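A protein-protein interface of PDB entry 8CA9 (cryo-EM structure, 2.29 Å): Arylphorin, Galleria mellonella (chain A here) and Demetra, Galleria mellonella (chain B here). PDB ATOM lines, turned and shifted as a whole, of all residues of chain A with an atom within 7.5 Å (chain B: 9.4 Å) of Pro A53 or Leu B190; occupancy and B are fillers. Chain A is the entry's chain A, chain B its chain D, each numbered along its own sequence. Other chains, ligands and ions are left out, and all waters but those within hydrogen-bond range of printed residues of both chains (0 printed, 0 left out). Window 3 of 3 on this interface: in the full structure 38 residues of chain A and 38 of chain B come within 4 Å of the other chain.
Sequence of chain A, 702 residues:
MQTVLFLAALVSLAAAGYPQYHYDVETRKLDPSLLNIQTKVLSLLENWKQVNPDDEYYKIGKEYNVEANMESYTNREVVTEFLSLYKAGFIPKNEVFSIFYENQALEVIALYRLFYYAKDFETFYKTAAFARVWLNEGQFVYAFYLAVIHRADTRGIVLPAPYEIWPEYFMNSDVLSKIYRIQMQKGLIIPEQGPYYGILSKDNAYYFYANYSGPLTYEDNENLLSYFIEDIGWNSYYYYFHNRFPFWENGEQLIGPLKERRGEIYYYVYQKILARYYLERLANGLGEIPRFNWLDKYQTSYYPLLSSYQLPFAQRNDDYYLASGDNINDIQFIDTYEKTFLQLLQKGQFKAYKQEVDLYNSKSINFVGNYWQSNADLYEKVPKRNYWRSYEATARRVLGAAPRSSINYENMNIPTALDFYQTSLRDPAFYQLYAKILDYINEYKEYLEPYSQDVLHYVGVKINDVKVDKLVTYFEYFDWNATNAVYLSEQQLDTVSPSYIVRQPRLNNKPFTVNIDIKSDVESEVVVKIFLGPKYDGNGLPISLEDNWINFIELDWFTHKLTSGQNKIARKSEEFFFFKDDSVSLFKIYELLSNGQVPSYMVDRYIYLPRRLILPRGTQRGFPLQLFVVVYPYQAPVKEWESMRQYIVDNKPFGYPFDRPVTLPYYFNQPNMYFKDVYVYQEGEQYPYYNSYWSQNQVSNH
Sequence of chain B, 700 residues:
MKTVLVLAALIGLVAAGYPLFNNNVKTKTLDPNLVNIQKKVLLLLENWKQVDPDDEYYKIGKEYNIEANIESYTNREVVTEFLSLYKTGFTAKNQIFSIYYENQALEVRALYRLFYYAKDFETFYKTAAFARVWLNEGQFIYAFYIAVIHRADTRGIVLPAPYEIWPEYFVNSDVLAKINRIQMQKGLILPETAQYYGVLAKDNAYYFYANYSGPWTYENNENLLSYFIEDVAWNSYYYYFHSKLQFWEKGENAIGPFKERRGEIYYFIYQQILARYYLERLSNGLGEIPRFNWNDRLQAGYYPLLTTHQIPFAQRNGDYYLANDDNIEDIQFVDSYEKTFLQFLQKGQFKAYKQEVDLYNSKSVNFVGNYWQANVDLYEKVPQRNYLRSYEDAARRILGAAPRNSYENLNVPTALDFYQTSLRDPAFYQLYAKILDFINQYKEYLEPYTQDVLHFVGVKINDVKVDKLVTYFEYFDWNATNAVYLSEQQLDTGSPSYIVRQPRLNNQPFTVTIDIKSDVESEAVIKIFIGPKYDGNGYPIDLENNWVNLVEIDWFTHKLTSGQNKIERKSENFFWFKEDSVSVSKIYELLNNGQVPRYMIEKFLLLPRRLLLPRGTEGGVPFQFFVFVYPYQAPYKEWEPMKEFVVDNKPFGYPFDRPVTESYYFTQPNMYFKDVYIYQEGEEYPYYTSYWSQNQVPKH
The side-chain amide oxygen of Gln B185 lies within hydrogen-bond range of the side-chain amide nitrogen of Gln A50, at 2.6 Å.
Printed residues of chain B that touch a printed residue of chain A: Gln B185, Ile B189 and Leu B190. Hydrophobic or aromatic side chains of chain B within 4 Å of the printed part of chain A: Ile B189 and Leu B190. Among the printed residues, 4 pairs touch across the chains. Among the printed residues, no Asp or Glu carboxylate lies within 4 Å of a Lys or Arg side-chain nitrogen of the other chain.
Among the printed residues, pairs that only touch across the chains: Glu A490 with Ile B189, Pro A53 with Leu B190 and Val A51 with Leu B190.
Of the printed residues of chain B, Pro A53 touches Leu B190. Leu B190 touches just these residues of chain A: Val A51 and Pro A53. No residue of chain B comes within 4 Å of Asp A54. Printed residues of chain B within 4 Å of Gln A50: Gln B185. Of the printed residues of chain B, Glu A490 touches Ile B189 (3.6 Å). Printed residues of chain A within 4 Å of Gln B185: Gln A50. Of the printed residues of chain B, Val A51 touches Leu B190. Tyr A58 touches none of the printed residues of chain B. The nearest residue of chain B that does not touch Pro A53 is Ile B189 (4.2 Å).
The guanidinium group of Arg B181 is in hydrogen-bond range of the side-chain amide oxygen of Gln B185 (3.3 Å). The side-chain amide nitrogen (NE2) of Gln B185 lies close to the backbone carbonyl oxygen (O) of Gly B187, at 3.4 Å. The side-chain hydroxyl of Thr B193 sits at hydrogen-bond distance from the backbone carbonyl oxygen of Leu B190 (2.8 Å).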
ATOM      1  N   GLN A  50      21.709 -17.640  19.081  1.00  0.00           N
ATOM      2  CA  GLN A  50      21.077 -16.540  19.793  1.00  0.00           C
ATOM      3  C   GLN A  50      21.774 -15.231  19.454  1.00  0.00           C
ATOM      4  O   GLN A  50      22.955 -15.209  19.097  1.00  0.00           O
ATOM      5  CB  GLN A  50      21.114 -16.761  21.311  1.00  0.00           C
ATOM      6  CG  GLN A  50      20.449 -18.046  21.769  1.00  0.00           C
ATOM      7  CD  GLN A  50      20.596 -18.275  23.258  1.00  0.00           C
ATOM      8  OE1 GLN A  50      21.519 -18.957  23.705  1.00  0.00           O
ATOM      9  NE2 GLN A  50      19.686 -17.704  24.037  1.00  0.00           N
ATOM     10  N   VAL A  51      21.024 -14.138  19.571  1.00  0.00           N
ATOM     11  CA  VAL A  51      21.532 -12.790  19.342  1.00  0.00           C
ATOM     12  C   VAL A  51      21.556 -12.067  20.682  1.00  0.00           C
ATOM     13  O   VAL A  51      20.524 -11.958  21.355  1.00  0.00           O
ATOM     14  CB  VAL A  51      20.675 -12.028  18.319  1.00  0.00           C
ATOM     15  CG1 VAL A  51      21.177 -10.601  18.160  1.00  0.00           C
ATOM     16  CG2 VAL A  51      20.679 -12.750  16.980  1.00  0.00           C
ATOM     17  N   ASN A  52      22.733 -11.573  21.068  1.00  0.00           N
ATOM     18  CA  ASN A  52      22.896 -10.864  22.329  1.00  0.00           C
ATOM     19  C   ASN A  52      22.925  -9.367  22.067  1.00  0.00           C
ATOM     20  O   ASN A  52      23.862  -8.888  21.410  1.00  0.00           O
ATOM     21  CB  ASN A  52      24.179 -11.301  23.027  1.00  0.00           C
ATOM     22  CG  ASN A  52      24.308 -10.730  24.427  1.00  0.00           C
ATOM     23  OD1 ASN A  52      23.608  -9.787  24.793  1.00  0.00           O
ATOM     24  ND2 ASN A  52      25.213 -11.298  25.214  1.00  0.00           N
ATOM     25  N   PRO A  53      21.948  -8.592  22.547  1.00  0.00           N
ATOM     26  CA  PRO A  53      21.964  -7.148  22.260  1.00  0.00           C
ATOM     27  C   PRO A  53      23.157  -6.414  22.851  1.00  0.00           C
ATOM     28  O   PRO A  53      23.488  -5.318  22.380  1.00  0.00           O
ATOM     29  CB  PRO A  53      20.639  -6.662  22.864  1.00  0.00           C
ATOM     30  CG  PRO A  53      20.332  -7.653  23.931  1.00  0.00           C
ATOM     31  CD  PRO A  53      20.792  -8.967  23.378  1.00  0.00           C
ATOM     32  N   ASP A  54      23.809  -6.973  23.871  1.00  0.00           N
ATOM     33  CA  ASP A  54      24.924  -6.297  24.523  1.00  0.00           C
ATOM     34  C   ASP A  54      26.228  -6.392  23.742  1.00  0.00           C
ATOM     35  O   ASP A  54      27.204  -5.735  24.120  1.00  0.00           O
ATOM     36  CB  ASP A  54      25.139  -6.868  25.929  1.00  0.00           C
ATOM     37  CG  ASP A  54      24.101  -6.381  26.921  1.00  0.00           C
ATOM     38  OD1 ASP A  54      23.728  -5.190  26.858  1.00  0.00           O
ATOM     39  OD2 ASP A  54      23.658  -7.190  27.765  1.00  0.00           O
ATOM     40  N   ASP A  55      26.277  -7.186  22.675  1.00  0.00           N
ATOM     41  CA  ASP A  55      27.509  -7.349  21.921  1.00  0.00           C
ATOM     42  C   ASP A  55      27.665  -6.241  20.880  1.00  0.00           C
ATOM     43  O   ASP A  55      26.694  -5.639  20.416  1.00  0.00           O
ATOM     44  CB  ASP A  55      27.545  -8.715  21.237  1.00  0.00           C
ATOM     45  CG  ASP A  55      27.737  -9.855  22.219  1.00  0.00           C
ATOM     46  OD1 ASP A  55      28.363  -9.632  23.278  1.00  0.00           O
ATOM     47  OD2 ASP A  55      27.268 -10.975  21.930  1.00  0.00           O
ATOM     48  N   GLU A  56      28.924  -5.983  20.516  1.00  0.00           N
ATOM     49  CA  GLU A  56      29.227  -4.956  19.524  1.00  0.00           C
ATOM     50  C   GLU A  56      28.612  -5.292  18.170  1.00  0.00           C
ATOM     51  O   GLU A  56      28.072  -4.411  17.484  1.00  0.00           O
ATOM     52  CB  GLU A  56      30.745  -4.801  19.409  1.00  0.00           C
ATOM     53  CG  GLU A  56      31.226  -3.954  18.243  1.00  0.00           C
ATOM     54  CD  GLU A  56      32.741  -3.883  18.170  1.00  0.00           C
ATOM     55  OE1 GLU A  56      33.403  -4.291  19.147  1.00  0.00           O
ATOM     56  OE2 GLU A  56      33.270  -3.427  17.134  1.00  0.00           O
ATOM     57  N   TYR A  57      28.687  -6.565  17.767  1.00  0.00           N
ATOM     58  CA  TYR A  57      28.154  -6.951  16.467  1.00  0.00           C
ATOM     59  C   TYR A  57      26.677  -6.609  16.352  1.00  0.00           C
ATOM     60  O   TYR A  57      26.198  -6.309  15.256  1.00  0.00           O
ATOM     61  CB  TYR A  57      28.378  -8.446  16.218  1.00  0.00           C
ATOM     62  CG  TYR A  57      27.433  -9.366  16.966  1.00  0.00           C
ATOM     63  CD1 TYR A  57      26.159  -9.633  16.480  1.00  0.00           C
ATOM     64  CD2 TYR A  57      27.825  -9.983  18.145  1.00  0.00           C
ATOM     65  CE1 TYR A  57      25.297 -10.472  17.158  1.00  0.00           C
ATOM     66  CE2 TYR A  57      26.970 -10.829  18.826  1.00  0.00           C
ATOM     67  CZ  TYR A  57      25.708 -11.069  18.328  1.00  0.00           C
ATOM     68  OH  TYR A  57      24.853 -11.909  19.003  1.00  0.00           O
ATOM     69  N   TYR A  58      25.942  -6.640  17.464  1.00  0.00           N
ATOM     70  CA  TYR A  58      24.522  -6.305  17.408  1.00  0.00           C
ATOM     71  C   TYR A  58      24.319  -4.884  16.905  1.00  0.00           C
ATOM     72  O   TYR A  58      23.568  -4.652  15.951  1.00  0.00           O
ATOM     73  CB  TYR A  58      23.885  -6.483  18.786  1.00  0.00           C
ATOM     74  CG  TYR A  58      22.417  -6.124  18.822  1.00  0.00           C
ATOM     75  CD1 TYR A  58      21.451  -7.035  18.416  1.00  0.00           C
ATOM     76  CD2 TYR A  58      21.996  -4.878  19.267  1.00  0.00           C
ATOM     77  CE1 TYR A  58      20.109  -6.714  18.449  1.00  0.00           C
ATOM     78  CE2 TYR A  58      20.656  -4.548  19.303  1.00  0.00           C
ATOM     79  CZ  TYR A  58      19.716  -5.469  18.893  1.00  0.00           C
ATOM     80  OH  TYR A  58      18.379  -5.147  18.926  1.00  0.00           O
ATOM     81  N   LYS A  59      24.993  -3.916  17.529  1.00  0.00           N
ATOM     82  CA  LYS A  59      24.867  -2.529  17.095  1.00  0.00           C
ATOM     83  C   LYS A  59      25.390  -2.356  15.674  1.00  0.00           C
ATOM     84  O   LYS A  59      24.761  -1.685  14.842  1.00  0.00           O
ATOM     85  CB  LYS A  59      25.614  -1.611  18.066  1.00  0.00           C
ATOM     86  CG  LYS A  59      25.188  -0.150  17.992  1.00  0.00           C
ATOM     87  CD  LYS A  59      26.064   0.747  18.863  1.00  0.00           C
ATOM     88  CE  LYS A  59      25.867   0.481  20.351  1.00  0.00           C
ATOM     89  NZ  LYS A  59      24.480   0.780  20.809  1.00  0.00           N
ATOM     90  N   LYS A  62      22.859  -3.766  13.289  1.00  0.00           N
ATOM     91  CA  LYS A  62      21.626  -2.990  13.300  1.00  0.00           C
ATOM     92  C   LYS A  62      21.777  -1.691  12.522  1.00  0.00           C
ATOM     93  O   LYS A  62      20.832  -1.255  11.854  1.00  0.00           O
ATOM     94  CB  LYS A  62      21.203  -2.694  14.741  1.00  0.00           C
ATOM     95  CG  LYS A  62      20.025  -3.526  15.233  1.00  0.00           C
ATOM     96  CD  LYS A  62      18.708  -3.009  14.675  1.00  0.00           C
ATOM     97  CE  LYS A  62      17.518  -3.780  15.232  1.00  0.00           C
ATOM     98  NZ  LYS A  62      17.533  -5.217  14.842  1.00  0.00           N
ATOM     99  N   VAL A 133      22.519 -10.398  12.736  1.00  0.00           N
ATOM    100  CA  VAL A 133      21.462  -9.651  13.407  1.00  0.00           C
ATOM    101  C   VAL A 133      20.126  -9.827  12.694  1.00  0.00           C
ATOM    102  O   VAL A 133      19.079  -9.915  13.347  1.00  0.00           O
ATOM    103  CB  VAL A 133      21.845  -8.164  13.516  1.00  0.00           C
ATOM    104  CG1 VAL A 133      20.661  -7.347  14.008  1.00  0.00           C
ATOM    105  CG2 VAL A 133      23.035  -7.989  14.450  1.00  0.00           C
ATOM    106  N   GLU A 490      20.334 -14.728  30.016  1.00  0.00           N
ATOM    107  CA  GLU A 490      21.005 -13.436  29.919  1.00  0.00           C
ATOM    108  C   GLU A 490      22.253 -13.407  30.792  1.00  0.00           C
ATOM    109  O   GLU A 490      23.316 -12.944  30.364  1.00  0.00           O
ATOM    110  CB  GLU A 490      20.034 -12.322  30.318  1.00  0.00           C
ATOM    111  CG  GLU A 490      20.611 -10.912  30.248  1.00  0.00           C
ATOM    112  CD  GLU A 490      19.580  -9.844  30.576  1.00  0.00           C
ATOM    113  OE1 GLU A 490      18.414 -10.200  30.845  1.00  0.00           O
ATOM    114  OE2 GLU A 490      19.936  -8.645  30.561  1.00  0.00           O
ATOM    115  N   LEU A 493      25.045 -15.462  29.262  1.00  0.00           N
ATOM    116  CA  LEU A 493      25.646 -14.726  28.158  1.00  0.00           C
ATOM    117  C   LEU A 493      26.559 -13.620  28.674  1.00  0.00           C
ATOM    118  O   LEU A 493      27.633 -13.379  28.113  1.00  0.00           O
ATOM    119  CB  LEU A 493      24.550 -14.138  27.265  1.00  0.00           C
ATOM    120  CG  LEU A 493      23.734 -15.139  26.439  1.00  0.00           C
ATOM    121  CD1 LEU A 493      22.490 -14.480  25.861  1.00  0.00           C
ATOM    122  CD2 LEU A 493      24.584 -15.734  25.330  1.00  0.00           C
ATOM    123  N   ASP A 494      26.140 -12.931  29.736  1.00  0.00           N
ATOM    124  CA  ASP A 494      26.917 -11.808  30.251  1.00  0.00           C
ATOM    125  C   ASP A 494      28.222 -12.270  30.885  1.00  0.00           C
ATOM    126  O   ASP A 494      29.300 -11.761  30.554  1.00  0.00           O
ATOM    127  CB  ASP A 494      26.090 -11.029  31.272  1.00  0.00           C
ATOM    128  CG  ASP A 494      24.874 -10.376  30.654  1.00  0.00           C
ATOM    129  OD1 ASP A 494      24.691 -10.502  29.429  1.00  0.00           O
ATOM    130  OD2 ASP A 494      24.103  -9.731  31.400  1.00  0.00           O
ATOM    131  N   ARG B 181      12.700 -23.758  25.248  1.00  0.00           N
ATOM    132  CA  ARG B 181      13.645 -22.663  25.062  1.00  0.00           C
ATOM    133  C   ARG B 181      13.430 -21.576  26.106  1.00  0.00           C
ATOM    134  O   ARG B 181      14.394 -21.051  26.675  1.00  0.00           O
ATOM    135  CB  ARG B 181      13.514 -22.081  23.654  1.00  0.00           C
ATOM    136  CG  ARG B 181      14.420 -20.885  23.408  1.00  0.00           C
ATOM    137  CD  ARG B 181      14.396 -20.440  21.959  1.00  0.00           C
ATOM    138  NE  ARG B 181      15.284 -19.308  21.728  1.00  0.00           N
ATOM    139  CZ  ARG B 181      15.513 -18.761  20.542  1.00  0.00           C
ATOM    140  NH1 ARG B 181      14.934 -19.222  19.445  1.00  0.00           N
ATOM    141  NH2 ARG B 181      16.344 -17.727  20.454  1.00  0.00           N
ATOM    142  N   ILE B 182      12.170 -21.227  26.375  1.00  0.00           N
ATOM    143  CA  ILE B 182      11.895 -20.211  27.389  1.00  0.00           C
ATOM    144  C   ILE B 182      12.384 -20.682  28.753  1.00  0.00           C
ATOM    145  O   ILE B 182      12.979 -19.910  29.515  1.00  0.00           O
ATOM    146  CB  ILE B 182      10.395 -19.863  27.416  1.00  0.00           C
ATOM    147  CG1 ILE B 182       9.957 -19.236  26.089  1.00  0.00           C
ATOM    148  CG2 ILE B 182      10.087 -18.924  28.575  1.00  0.00           C
ATOM    149  CD1 ILE B 182      10.707 -17.974  25.712  1.00  0.00           C
ATOM    150  N   GLN B 185      16.200 -20.443  28.880  1.00  0.00           N
ATOM    151  CA  GLN B 185      16.631 -19.053  28.948  1.00  0.00           C
ATOM    152  C   GLN B 185      16.118 -18.330  30.185  1.00  0.00           C
ATOM    153  O   GLN B 185      16.562 -17.209  30.455  1.00  0.00           O
ATOM    154  CB  GLN B 185      16.172 -18.297  27.698  1.00  0.00           C
ATOM    155  CG  GLN B 185      16.743 -18.839  26.396  1.00  0.00           C
ATOM    156  CD  GLN B 185      16.358 -18.012  25.179  1.00  0.00           C
ATOM    157  OE1 GLN B 185      17.073 -18.003  24.177  1.00  0.00           O
ATOM    158  NE2 GLN B 185      15.223 -17.322  25.254  1.00  0.00           N
ATOM    159  N   GLY B 187      13.363 -16.876  30.618  1.00  0.00           N
ATOM    160  CA  GLY B 187      12.711 -15.675  30.150  1.00  0.00           C
ATOM    161  C   GLY B 187      13.088 -15.381  28.717  1.00  0.00           C
ATOM    162  O   GLY B 187      13.588 -16.250  27.993  1.00  0.00           O
ATOM    163  N   LEU B 188      12.842 -14.141  28.305  1.00  0.00           N
ATOM    164  CA  LEU B 188      13.120 -13.687  26.951  1.00  0.00           C
ATOM    165  C   LEU B 188      14.355 -12.795  26.939  1.00  0.00           C
ATOM    166  O   LEU B 188      14.507 -11.914  27.789  1.00  0.00           O
ATOM    167  CB  LEU B 188      11.925 -12.921  26.379  1.00  0.00           C
ATOM    168  CG  LEU B 188      10.642 -13.730  26.177  1.00  0.00           C
ATOM    169  CD1 LEU B 188       9.472 -12.807  25.886  1.00  0.00           C
ATOM    170  CD2 LEU B 188      10.817 -14.739  25.053  1.00  0.00           C
ATOM    171  N   ILE B 189      15.234 -13.031  25.969  1.00  0.00           N
ATOM    172  CA  ILE B 189      16.428 -12.207  25.810  1.00  0.00           C
ATOM    173  C   ILE B 189      16.105 -10.906  25.088  1.00  0.00           C
ATOM    174  O   ILE B 189      16.628  -9.847  25.440  1.00  0.00           O
ATOM    175  CB  ILE B 189      17.523 -13.003  25.066  1.00  0.00           C
ATOM    176  CG1 ILE B 189      17.728 -14.382  25.704  1.00  0.00           C
ATOM    177  CG2 ILE B 189      18.830 -12.226  25.056  1.00  0.00           C
ATOM    178  CD1 ILE B 189      18.173 -14.347  27.151  1.00  0.00           C
ATOM    179  N   LEU B 190      15.242 -10.972  24.070  1.00  0.00           N
ATOM    180  CA  LEU B 190      14.785  -9.809  23.312  1.00  0.00           C
ATOM    181  C   LEU B 190      13.261  -9.841  23.308  1.00  0.00           C
ATOM    182  O   LEU B 190      12.641 -10.269  22.323  1.00  0.00           O
ATOM    183  CB  LEU B 190      15.350  -9.815  21.893  1.00  0.00           C
ATOM    184  CG  LEU B 190      16.869  -9.656  21.799  1.00  0.00           C
ATOM    185  CD1 LEU B 190      17.376 -10.141  20.452  1.00  0.00           C
ATOM    186  CD2 LEU B 190      17.271  -8.208  22.026  1.00  0.00           C
ATOM    187  N   PRO B 191      12.621  -9.398  24.395  1.00  0.00           N
ATOM    188  CA  PRO B 191      11.165  -9.596  24.511  1.00  0.00           C
ATOM    189  C   PRO B 191      10.363  -8.968  23.386  1.00  0.00           C
ATOM    190  O   PRO B 191       9.379  -9.564  22.928  1.00  0.00           O
ATOM    191  CB  PRO B 191      10.836  -8.957  25.870  1.00  0.00           C
ATOM    192  CG  PRO B 191      11.949  -8.006  26.133  1.00  0.00           C
ATOM    193  CD  PRO B 191      13.166  -8.622  25.523  1.00  0.00           C
ATOM    194  N   GLU B 192      10.765  -7.791  22.904  1.00  0.00           N
ATOM    195  CA  GLU B 192       9.956  -7.061  21.935  1.00  0.00           C
ATOM    196  C   GLU B 192       9.782  -7.805  20.617  1.00  0.00           C
ATOM    197  O   GLU B 192       8.977  -7.366  19.788  1.00  0.00           O
ATOM    198  CB  GLU B 192      10.564  -5.680  21.665  1.00  0.00           C
ATOM    199  CG  GLU B 192      11.917  -5.689  20.954  1.00  0.00           C
ATOM    200  CD  GLU B 192      13.068  -6.064  21.870  1.00  0.00           C
ATOM    201  OE1 GLU B 192      12.857  -6.124  23.101  1.00  0.00           O
ATOM    202  OE2 GLU B 192      14.182  -6.300  21.360  1.00  0.00           O
ATOM    203  N   THR B 193      10.499  -8.909  20.402  1.00  0.00           N
ATOM    204  CA  THR B 193      10.340  -9.714  19.201  1.00  0.00           C
ATOM    205  C   THR B 193       9.574 -11.006  19.442  1.00  0.00           C
ATOM    206  O   THR B 193       9.078 -11.599  18.477  1.00  0.00           O
ATOM    207  CB  THR B 193      11.713 -10.057  18.601  1.00  0.00           C
ATOM    208  OG1 THR B 193      12.478 -10.811  19.548  1.00  0.00           O
ATOM    209  CG2 THR B 193      12.472  -8.792  18.230  1.00  0.00           C
ATOM    210  N   ALA B 194       9.448 -11.449  20.696  1.00  0.00           N
ATOM    211  CA  ALA B 194       8.766 -12.709  20.967  1.00  0.00           C
ATOM    212  C   ALA B 194       7.345 -12.705  20.421  1.00  0.00           C
ATOM    213  O   ALA B 194       6.830 -13.755  20.020  1.00  0.00           O
ATOM    214  CB  ALA B 194       8.759 -12.989  22.469  1.00  0.00           C
ATOM    215  N   GLN B 195       6.700 -11.536  20.389  1.00  0.00           N
ATOM    216  CA  GLN B 195       5.344 -11.451  19.863  1.00  0.00           C
ATOM    217  C   GLN B 195       5.260 -11.986  18.441  1.00  0.00           C
ATOM    218  O   GLN B 195       4.266 -12.621  18.073  1.00  0.00           O
ATOM    219  CB  GLN B 195       4.859 -10.001  19.904  1.00  0.00           C
ATOM    220  CG  GLN B 195       4.834  -9.386  21.294  1.00  0.00           C
ATOM    221  CD  GLN B 195       4.902  -7.871  21.257  1.00  0.00           C
ATOM    222  OE1 GLN B 195       5.686  -7.292  20.506  1.00  0.00           O
ATOM    223  NE2 GLN B 195       4.075  -7.221  22.068  1.00  0.00           N
ATOM    224  N   TYR B 196       6.291 -11.744  17.629  1.00  0.00           N
ATOM    225  CA  TYR B 196       6.275 -12.188  16.241  1.00  0.00           C
ATOM    226  C   TYR B 196       6.431 -13.695  16.101  1.00  0.00           C
ATOM    227  O   TYR B 196       6.247 -14.216  14.996  1.00  0.00           O
ATOM    228  CB  TYR B 196       7.378 -11.474  15.457  1.00  0.00           C
ATOM    229  CG  TYR B 196       7.184  -9.976  15.378  1.00  0.00           C
ATOM    230  CD1 TYR B 196       6.342  -9.414  14.428  1.00  0.00           C
ATOM    231  CD2 TYR B 196       7.837  -9.124  16.257  1.00  0.00           C
ATOM    232  CE1 TYR B 196       6.159  -8.048  14.353  1.00  0.00           C
ATOM    233  CE2 TYR B 196       7.661  -7.754  16.190  1.00  0.00           C
ATOM    234  CZ  TYR B 196       6.819  -7.222  15.236  1.00  0.00           C
ATOM    235  OH  TYR B 196       6.639  -5.860  15.165  1.00  0.00           O
ATOM    236  N   TYR B 197       6.763 -14.405  17.182  1.00  0.00           N
ATOM    237  CA  TYR B 197       6.897 -15.857  17.155  1.00  0.00           C
ATOM    238  C   TYR B 197       5.845 -16.542  18.020  1.00  0.00           C
ATOM    239  O   TYR B 197       6.036 -17.687  18.435  1.00  0.00           O
ATOM    240  CB  TYR B 197       8.302 -16.268  17.598  1.00  0.00           C
ATOM    241  CG  TYR B 197       9.399 -15.618  16.786  1.00  0.00           C
ATOM    242  CD1 TYR B 197       9.993 -14.437  17.205  1.00  0.00           C
ATOM    243  CD2 TYR B 197       9.835 -16.181  15.593  1.00  0.00           C
ATOM    244  CE1 TYR B 197      10.992 -13.837  16.467  1.00  0.00           C
ATOM    245  CE2 TYR B 197      10.834 -15.588  14.846  1.00  0.00           C
ATOM    246  CZ  TYR B 197      11.409 -14.416  15.288  1.00  0.00           C
ATOM    247  OH  TYR B 197      12.405 -13.822  14.547  1.00  0.00           O
ATOM    248  N   VAL B 199       4.747 -15.832  21.167  1.00  0.00           N
ATOM    249  CA  VAL B 199       5.105 -15.958  22.576  1.00  0.00           C
ATOM    250  C   VAL B 199       4.833 -14.612  23.232  1.00  0.00           C
ATOM    251  O   VAL B 199       5.507 -13.621  22.926  1.00  0.00           O
ATOM    252  CB  VAL B 199       6.569 -16.378  22.771  1.00  0.00           C
ATOM    253  CG1 VAL B 199       6.883 -16.520  24.250  1.00  0.00           C
ATOM    254  CG2 VAL B 199       6.850 -17.677  22.034  1.00  0.00           C
ATOM    255  N   ALA B 201       4.395 -12.382  26.816  1.00  0.00           N
ATOM    256  CA  ALA B 201       4.710 -12.291  28.236  1.00  0.00           C
ATOM    257  C   ALA B 201       3.722 -11.344  28.902  1.00  0.00           C
ATOM    258  O   ALA B 201       3.604 -10.182  28.496  1.00  0.00           O
ATOM    259  CB  ALA B 201       6.143 -11.800  28.451  1.00  0.00           C
